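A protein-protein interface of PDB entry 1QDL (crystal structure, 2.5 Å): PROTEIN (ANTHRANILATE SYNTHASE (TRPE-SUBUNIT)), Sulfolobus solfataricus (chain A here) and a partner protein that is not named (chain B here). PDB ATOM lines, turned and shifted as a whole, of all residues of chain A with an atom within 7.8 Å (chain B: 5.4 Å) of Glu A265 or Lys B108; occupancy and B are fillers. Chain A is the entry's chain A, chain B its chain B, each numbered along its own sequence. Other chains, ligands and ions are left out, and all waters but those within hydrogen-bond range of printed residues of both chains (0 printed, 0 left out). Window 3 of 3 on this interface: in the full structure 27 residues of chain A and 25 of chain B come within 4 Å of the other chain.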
ATOM      1  N   GLU A 260     -17.669   6.906  10.496  1.00  0.00           N
ATOM      2  CA  GLU A 260     -18.298   5.920   9.622  1.00  0.00           C
ATOM      3  C   GLU A 260     -18.728   6.695   8.398  1.00  0.00           C
ATOM      4  O   GLU A 260     -18.653   6.209   7.268  1.00  0.00           O
ATOM      5  CB  GLU A 260     -19.521   5.320  10.286  1.00  0.00           C
ATOM      6  CG  GLU A 260     -19.222   4.103  11.103  1.00  0.00           C
ATOM      7  CD  GLU A 260     -20.476   3.342  11.429  1.00  0.00           C
ATOM      8  OE1 GLU A 260     -20.768   2.354  10.719  1.00  0.00           O
ATOM      9  OE2 GLU A 260     -21.172   3.744  12.385  1.00  0.00           O
ATOM     10  N   LEU A 261     -19.191   7.913   8.652  1.00  0.00           N
ATOM     11  CA  LEU A 261     -19.614   8.811   7.597  1.00  0.00           C
ATOM     12  C   LEU A 261     -18.375   9.162   6.790  1.00  0.00           C
ATOM     13  O   LEU A 261     -18.350   9.013   5.573  1.00  0.00           O
ATOM     14  CB  LEU A 261     -20.203  10.081   8.199  1.00  0.00           C
ATOM     15  CG  LEU A 261     -21.597   9.940   8.795  1.00  0.00           C
ATOM     16  CD1 LEU A 261     -21.997  11.229   9.493  1.00  0.00           C
ATOM     17  CD2 LEU A 261     -22.568   9.583   7.685  1.00  0.00           C
ATOM     18  N   MET A 262     -17.342   9.620   7.486  1.00  0.00           N
ATOM     19  CA  MET A 262     -16.086  10.001   6.862  1.00  0.00           C
ATOM     20  C   MET A 262     -15.535   8.915   5.934  1.00  0.00           C
ATOM     21  O   MET A 262     -14.882   9.202   4.937  1.00  0.00           O
ATOM     22  CB  MET A 262     -15.055  10.290   7.949  1.00  0.00           C
ATOM     23  CG  MET A 262     -14.851  11.759   8.303  1.00  0.00           C
ATOM     24  SD  MET A 262     -13.369  12.005   9.356  1.00  0.00           S
ATOM     25  CE  MET A 262     -12.435  13.251   8.391  1.00  0.00           C
ATOM     26  N   ASN A 263     -15.801   7.660   6.256  1.00  0.00           N
ATOM     27  CA  ASN A 263     -15.268   6.568   5.448  1.00  0.00           C
ATOM     28  C   ASN A 263     -16.269   5.911   4.513  1.00  0.00           C
ATOM     29  O   ASN A 263     -15.935   4.958   3.803  1.00  0.00           O
ATOM     30  CB  ASN A 263     -14.662   5.511   6.368  1.00  0.00           C
ATOM     31  CG  ASN A 263     -13.434   6.015   7.093  1.00  0.00           C
ATOM     32  OD1 ASN A 263     -12.432   6.350   6.464  1.00  0.00           O
ATOM     33  ND2 ASN A 263     -13.505   6.081   8.417  1.00  0.00           N
ATOM     34  N   SER A 264     -17.495   6.420   4.517  1.00  0.00           N
ATOM     35  CA  SER A 264     -18.552   5.883   3.674  1.00  0.00           C
ATOM     36  C   SER A 264     -18.355   6.290   2.223  1.00  0.00           C
ATOM     37  O   SER A 264     -18.650   7.414   1.837  1.00  0.00           O
ATOM     38  CB  SER A 264     -19.909   6.379   4.164  1.00  0.00           C
ATOM     39  OG  SER A 264     -20.957   5.696   3.504  1.00  0.00           O
ATOM     40  N   GLU A 265     -17.844   5.368   1.423  1.00  0.00           N
ATOM     41  CA  GLU A 265     -17.617   5.617   0.011  1.00  0.00           C
ATOM     42  C   GLU A 265     -18.959   5.996  -0.613  1.00  0.00           C
ATOM     43  O   GLU A 265     -19.048   6.897  -1.449  1.00  0.00           O
ATOM     44  CB  GLU A 265     -17.062   4.347  -0.637  1.00  0.00           C
ATOM     45  CG  GLU A 265     -16.516   4.515  -2.045  1.00  0.00           C
ATOM     46  CD  GLU A 265     -16.649   3.242  -2.878  1.00  0.00           C
ATOM     47  OE1 GLU A 265     -17.339   2.304  -2.410  1.00  0.00           O
ATOM     48  OE2 GLU A 265     -16.073   3.175  -3.993  1.00  0.00           O
ATOM     49  N   LYS A 266     -20.010   5.312  -0.176  1.00  0.00           N
ATOM     50  CA  LYS A 266     -21.350   5.550  -0.686  1.00  0.00           C
ATOM     51  C   LYS A 266     -21.904   6.920  -0.293  1.00  0.00           C
ATOM     52  O   LYS A 266     -22.293   7.710  -1.153  1.00  0.00           O
ATOM     53  CB  LYS A 266     -22.287   4.433  -0.196  1.00  0.00           C
ATOM     54  CG  LYS A 266     -23.735   4.864   0.062  1.00  0.00           C
ATOM     55  CD  LYS A 266     -24.586   3.737   0.652  1.00  0.00           C
ATOM     56  CE  LYS A 266     -26.075   3.915   0.318  1.00  0.00           C
ATOM     57  NZ  LYS A 266     -26.615   2.849  -0.593  1.00  0.00           N
ATOM     58  N   ASP A 267     -21.941   7.201   1.003  1.00  0.00           N
ATOM     59  CA  ASP A 267     -22.475   8.464   1.490  1.00  0.00           C
ATOM     60  C   ASP A 267     -21.719   9.685   0.973  1.00  0.00           C
ATOM     61  O   ASP A 267     -22.298  10.761   0.826  1.00  0.00           O
ATOM     62  CB  ASP A 267     -22.481   8.481   3.021  1.00  0.00           C
ATOM     63  CG  ASP A 267     -23.604   7.647   3.614  1.00  0.00           C
ATOM     64  OD1 ASP A 267     -23.732   7.637   4.859  1.00  0.00           O
ATOM     65  OD2 ASP A 267     -24.354   7.005   2.843  1.00  0.00           O
ATOM     66  N   LYS A 268     -20.429   9.528   0.700  1.00  0.00           N
ATOM     67  CA  LYS A 268     -19.640  10.648   0.202  1.00  0.00           C
ATOM     68  C   LYS A 268     -19.975  10.914  -1.267  1.00  0.00           C
ATOM     69  O   LYS A 268     -20.108  12.068  -1.686  1.00  0.00           O
ATOM     70  CB  LYS A 268     -18.145  10.359   0.364  1.00  0.00           C
ATOM     71  CG  LYS A 268     -17.716  10.138   1.810  1.00  0.00           C
ATOM     72  CD  LYS A 268     -16.335  10.716   2.108  1.00  0.00           C
ATOM     73  CE  LYS A 268     -15.224   9.914   1.440  1.00  0.00           C
ATOM     74  NZ  LYS A 268     -15.120   8.510   1.933  1.00  0.00           N
ATOM     75  N   ALA A 269     -20.124   9.839  -2.040  1.00  0.00           N
ATOM     76  CA  ALA A 269     -20.447   9.950  -3.458  1.00  0.00           C
ATOM     77  C   ALA A 269     -21.748  10.716  -3.634  1.00  0.00           C
ATOM     78  O   ALA A 269     -21.837  11.623  -4.458  1.00  0.00           O
ATOM     79  CB  ALA A 269     -20.567   8.569  -4.077  1.00  0.00           C
ATOM     80  N   GLU A 270     -22.757  10.355  -2.853  1.00  0.00           N
ATOM     81  CA  GLU A 270     -24.039  11.032  -2.939  1.00  0.00           C
ATOM     82  C   GLU A 270     -23.883  12.494  -2.539  1.00  0.00           C
ATOM     83  O   GLU A 270     -24.545  13.371  -3.098  1.00  0.00           O
ATOM     84  CB  GLU A 270     -25.062  10.338  -2.031  1.00  0.00           C
ATOM     85  CG  GLU A 270     -25.991  11.293  -1.284  1.00  0.00           C
ATOM     86  CD  GLU A 270     -27.310  10.656  -0.871  1.00  0.00           C
ATOM     87  OE1 GLU A 270     -28.336  11.374  -0.839  1.00  0.00           O
ATOM     88  OE2 GLU A 270     -27.320   9.441  -0.576  1.00  0.00           O
ATOM     89  N   HIS A 271     -23.007  12.759  -1.569  1.00  0.00           N
ATOM     90  CA  HIS A 271     -22.787  14.125  -1.103  1.00  0.00           C
ATOM     91  C   HIS A 271     -22.097  14.969  -2.168  1.00  0.00           C
ATOM     92  O   HIS A 271     -22.477  16.120  -2.417  1.00  0.00           O
ATOM     93  CB  HIS A 271     -21.942  14.141   0.177  1.00  0.00           C
ATOM     94  CG  HIS A 271     -21.974  15.454   0.896  1.00  0.00           C
ATOM     95  ND1 HIS A 271     -21.000  16.417   0.738  1.00  0.00           N
ATOM     96  CD2 HIS A 271     -22.883  15.982   1.752  1.00  0.00           C
ATOM     97  CE1 HIS A 271     -21.306  17.478   1.463  1.00  0.00           C
ATOM     98  NE2 HIS A 271     -22.445  17.239   2.087  1.00  0.00           N
ATOM     99  N   LEU A 272     -21.076  14.386  -2.788  1.00  0.00           N
ATOM    100  CA  LEU A 272     -20.319  15.073  -3.822  1.00  0.00           C
ATOM    101  C   LEU A 272     -21.245  15.526  -4.937  1.00  0.00           C
ATOM    102  O   LEU A 272     -21.165  16.658  -5.412  1.00  0.00           O
ATOM    103  CB  LEU A 272     -19.246  14.151  -4.394  1.00  0.00           C
ATOM    104  CG  LEU A 272     -18.483  14.741  -5.581  1.00  0.00           C
ATOM    105  CD1 LEU A 272     -17.925  16.094  -5.194  1.00  0.00           C
ATOM    106  CD2 LEU A 272     -17.368  13.806  -6.009  1.00  0.00           C
ATOM    107  N   MET A 273     -22.124  14.628  -5.352  1.00  0.00           N
ATOM    108  CA  MET A 273     -23.067  14.934  -6.402  1.00  0.00           C
ATOM    109  C   MET A 273     -23.964  16.107  -6.002  1.00  0.00           C
ATOM    110  O   MET A 273     -24.242  16.995  -6.810  1.00  0.00           O
ATOM    111  CB  MET A 273     -23.915  13.703  -6.686  1.00  0.00           C
ATOM    112  CG  MET A 273     -25.071  13.942  -7.627  1.00  0.00           C
ATOM    113  SD  MET A 273     -26.170  12.533  -7.680  1.00  0.00           S
ATOM    114  CE  MET A 273     -27.333  12.918  -6.309  1.00  0.00           C
ATOM    115  N   ILE A 308     -22.998  14.452   6.757  1.00  0.00           N
ATOM    116  CA  ILE A 308     -21.862  15.017   6.047  1.00  0.00           C
ATOM    117  C   ILE A 308     -22.449  16.320   5.504  1.00  0.00           C
ATOM    118  O   ILE A 308     -23.547  16.320   4.940  1.00  0.00           O
ATOM    119  CB  ILE A 308     -21.463  14.156   4.851  1.00  0.00           C
ATOM    120  CG1 ILE A 308     -20.996  12.781   5.326  1.00  0.00           C
ATOM    121  CG2 ILE A 308     -20.413  14.882   4.023  1.00  0.00           C
ATOM    122  CD1 ILE A 308     -20.675  11.831   4.183  1.00  0.00           C
ATOM    123  N   TYR A 397     -28.324   3.536  -7.894  1.00  0.00           N
ATOM    124  CA  TYR A 397     -28.135   2.330  -8.670  1.00  0.00           C
ATOM    125  C   TYR A 397     -28.189   1.016  -7.920  1.00  0.00           C
ATOM    126  O   TYR A 397     -28.675   0.024  -8.460  1.00  0.00           O
ATOM    127  CB  TYR A 397     -26.850   2.432  -9.476  1.00  0.00           C
ATOM    128  CG  TYR A 397     -25.631   1.941  -8.766  1.00  0.00           C
ATOM    129  CD1 TYR A 397     -25.079   0.700  -9.075  1.00  0.00           C
ATOM    130  CD2 TYR A 397     -25.000   2.727  -7.808  1.00  0.00           C
ATOM    131  CE1 TYR A 397     -23.921   0.255  -8.450  1.00  0.00           C
ATOM    132  CE2 TYR A 397     -23.840   2.292  -7.176  1.00  0.00           C
ATOM    133  CZ  TYR A 397     -23.307   1.056  -7.503  1.00  0.00           C
ATOM    134  OH  TYR A 397     -22.157   0.626  -6.893  1.00  0.00           O
ATOM    135  N   ASP A 398     -27.712   0.993  -6.680  1.00  0.00           N
ATOM    136  CA  ASP A 398     -27.741  -0.244  -5.907  1.00  0.00           C
ATOM    137  C   ASP A 398     -28.697  -0.172  -4.721  1.00  0.00           C
ATOM    138  O   ASP A 398     -28.482  -0.809  -3.690  1.00  0.00           O
ATOM    139  CB  ASP A 398     -26.333  -0.602  -5.428  1.00  0.00           C
ATOM    140  CG  ASP A 398     -25.743   0.450  -4.517  1.00  0.00           C
ATOM    141  OD1 ASP A 398     -24.577   0.276  -4.100  1.00  0.00           O
ATOM    142  OD2 ASP A 398     -26.442   1.444  -4.216  1.00  0.00           O
ATOM    143  N   VAL B 104     -19.790   1.117 -11.950  1.00  0.00           N
ATOM    144  CA  VAL B 104     -20.595   2.342 -11.970  1.00  0.00           C
ATOM    145  C   VAL B 104     -20.109   3.458 -11.041  1.00  0.00           C
ATOM    146  O   VAL B 104     -20.265   3.391  -9.816  1.00  0.00           O
ATOM    147  CB  VAL B 104     -22.083   2.034 -11.633  1.00  0.00           C
ATOM    148  CG1 VAL B 104     -22.859   3.322 -11.384  1.00  0.00           C
ATOM    149  CG2 VAL B 104     -22.713   1.263 -12.770  1.00  0.00           C
ATOM    150  N   PHE B 105     -19.534   4.495 -11.640  1.00  0.00           N
ATOM    151  CA  PHE B 105     -19.043   5.638 -10.889  1.00  0.00           C
ATOM    152  C   PHE B 105     -20.048   6.760 -10.939  1.00  0.00           C
ATOM    153  O   PHE B 105     -20.171   7.461 -11.938  1.00  0.00           O
ATOM    154  CB  PHE B 105     -17.732   6.126 -11.466  1.00  0.00           C
ATOM    155  CG  PHE B 105     -16.569   5.299 -11.067  1.00  0.00           C
ATOM    156  CD1 PHE B 105     -16.494   3.960 -11.449  1.00  0.00           C
ATOM    157  CD2 PHE B 105     -15.543   5.847 -10.310  1.00  0.00           C
ATOM    158  CE1 PHE B 105     -15.409   3.175 -11.085  1.00  0.00           C
ATOM    159  CE2 PHE B 105     -14.455   5.076  -9.938  1.00  0.00           C
ATOM    160  CZ  PHE B 105     -14.387   3.733 -10.328  1.00  0.00           C
ATOM    161  N   HIS B 106     -20.779   6.925  -9.854  1.00  0.00           N
ATOM    162  CA  HIS B 106     -21.764   7.979  -9.797  1.00  0.00           C
ATOM    163  C   HIS B 106     -21.356   8.886  -8.659  1.00  0.00           C
ATOM    164  O   HIS B 106     -21.744   8.666  -7.515  1.00  0.00           O
ATOM    165  CB  HIS B 106     -23.147   7.394  -9.535  1.00  0.00           C
ATOM    166  CG  HIS B 106     -23.805   6.830 -10.753  1.00  0.00           C
ATOM    167  ND1 HIS B 106     -23.247   6.926 -12.009  1.00  0.00           N
ATOM    168  CD2 HIS B 106     -24.972   6.162 -10.908  1.00  0.00           C
ATOM    169  CE1 HIS B 106     -24.043   6.340 -12.886  1.00  0.00           C
ATOM    170  NE2 HIS B 106     -25.096   5.869 -12.243  1.00  0.00           N
ATOM    171  N   GLY B 107     -20.564   9.903  -8.973  1.00  0.00           N
ATOM    172  CA  GLY B 107     -20.113  10.819  -7.945  1.00  0.00           C
ATOM    173  C   GLY B 107     -18.865  10.277  -7.281  1.00  0.00           C
ATOM    174  O   GLY B 107     -18.437  10.781  -6.248  1.00  0.00           O
ATOM    175  N   LYS B 108     -18.290   9.236  -7.871  1.00  0.00           N
ATOM    176  CA  LYS B 108     -17.076   8.627  -7.340  1.00  0.00           C
ATOM    177  C   LYS B 108     -15.854   9.208  -8.047  1.00  0.00           C
ATOM    178  O   LYS B 108     -15.895   9.504  -9.242  1.00  0.00           O
ATOM    179  CB  LYS B 108     -17.121   7.105  -7.516  1.00  0.00           C
ATOM    180  CG  LYS B 108     -18.278   6.437  -6.771  1.00  0.00           C
ATOM    181  CD  LYS B 108     -17.868   5.119  -6.128  1.00  0.00           C
ATOM    182  CE  LYS B 108     -19.040   4.155  -6.088  1.00  0.00           C
ATOM    183  NZ  LYS B 108     -18.956   3.174  -7.204  1.00  0.00           N
ATOM    184  N   ILE B 109     -14.771   9.374  -7.293  1.00  0.00           N
ATOM    185  CA  ILE B 109     -13.527   9.927  -7.816  1.00  0.00           C
ATOM    186  C   ILE B 109     -12.611   8.832  -8.337  1.00  0.00           C
ATOM    187  O   ILE B 109     -12.281   7.895  -7.612  1.00  0.00           O
ATOM    188  CB  ILE B 109     -12.783  10.709  -6.731  1.00  0.00           C
ATOM    189  CG1 ILE B 109     -13.658  11.871  -6.255  1.00  0.00           C
ATOM    190  CG2 ILE B 109     -11.416  11.154  -7.250  1.00  0.00           C
ATOM    191  CD1 ILE B 109     -13.158  13.241  -6.646  1.00  0.00           C
ATOM    192  N   SER B 110     -12.193   8.959  -9.591  1.00  0.00           N
ATOM    193  CA  SER B 110     -11.323   7.969 -10.208  1.00  0.00           C
ATOM    194  C   SER B 110      -9.945   8.552 -10.497  1.00  0.00           C
ATOM    195  O   SER B 110      -9.768   9.770 -10.532  1.00  0.00           O
ATOM    196  CB  SER B 110     -11.956   7.459 -11.508  1.00  0.00           C
ATOM    197  OG  SER B 110     -11.547   6.138 -11.816  1.00  0.00           O
ATOM    198  N   ALA B 132     -10.246  12.664 -10.723  1.00  0.00           N
ATOM    199  CA  ALA B 132     -11.388  13.330 -11.333  1.00  0.00           C
ATOM    200  C   ALA B 132     -12.687  12.608 -10.990  1.00  0.00           C
ATOM    201  O   ALA B 132     -12.719  11.380 -10.844  1.00  0.00           O
ATOM    202  CB  ALA B 132     -11.209  13.389 -12.844  1.00  0.00           C
ATOM    203  N   THR B 133     -13.760  13.380 -10.859  1.00  0.00           N
ATOM    204  CA  THR B 133     -15.067  12.824 -10.541  1.00  0.00           C
ATOM    205  C   THR B 133     -15.668  12.143 -11.760  1.00  0.00           C
ATOM    206  O   THR B 133     -15.419  12.546 -12.895  1.00  0.00           O
ATOM    207  CB  THR B 133     -16.044  13.917 -10.091  1.00  0.00           C
ATOM    208  OG1 THR B 133     -15.399  14.772  -9.142  1.00  0.00           O
ATOM    209  CG2 THR B 133     -17.270  13.300  -9.453  1.00  0.00           C
ATOM    210  N   ARG B 134     -16.457  11.107 -11.517  1.00  0.00           N
ATOM    211  CA  ARG B 134     -17.119  10.390 -12.591  1.00  0.00           C
ATOM    212  C   ARG B 134     -18.591  10.302 -12.260  1.00  0.00           C
ATOM    213  O   ARG B 134     -18.962  10.118 -11.103  1.00  0.00           O
ATOM    214  CB  ARG B 134     -16.546   8.994 -12.735  1.00  0.00           C
ATOM    215  CG  ARG B 134     -15.296   8.951 -13.559  1.00  0.00           C
ATOM    216  CD  ARG B 134     -14.569   7.649 -13.342  1.00  0.00           C
ATOM    217  NE  ARG B 134     -15.260   6.538 -13.977  1.00  0.00           N
ATOM    218  CZ  ARG B 134     -14.778   5.302 -14.045  1.00  0.00           C
ATOM    219  NH1 ARG B 134     -15.477   4.343 -14.643  1.00  0.00           N
ATOM    220  NH2 ARG B 134     -13.595   5.024 -13.512  1.00  0.00           N
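O of Val B104 lies within hydrogen-bond range of NZ of Lys B108, 2.9 Å away.
The backbone NH of Gly B107 is in hydrogen-bond range of the backbone carbonyl oxygen of Arg B134.
The backbone NH (N) of Arg B134 sits at hydrogen-bond distance from the backbone carbonyl oxygen (O) of Lys B108.
Hydrophobic or aromatic side chains of chain A that line the printed part of chain B: Ala A269 and Leu A272.
Along chain A the printed residues that touch a printed residue of chain B span positions 265 to 272.
Among the printed residues, pairs that only touch across the chains: Leu A272 with Gly B107, Glu A265 with Lys B108, Leu A272 with Thr B133, Ala A269 with Gly B107 and Ala A269 with His B106.
Glu A265 touches one residue of chain B.
Of the printed residues of chain B, Ala A269 touches His B106 and Gly B107.
Printed residues of chain B within 4 Å of Leu A272: Gly B107 and Thr B133.
Of the printed residues of chain A, His B106 touches Ala A269 (3.6 Å).
Of chain A, only Glu A265 (3.4 Å) comes within 4 Å of Lys B108.
Of the printed residues of chain A, Thr B133 touches Leu A272 (3.5 Å).
The nearest printed residue of chain A that does not touch Lys B108 is Tyr A397 (4.1 Å).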
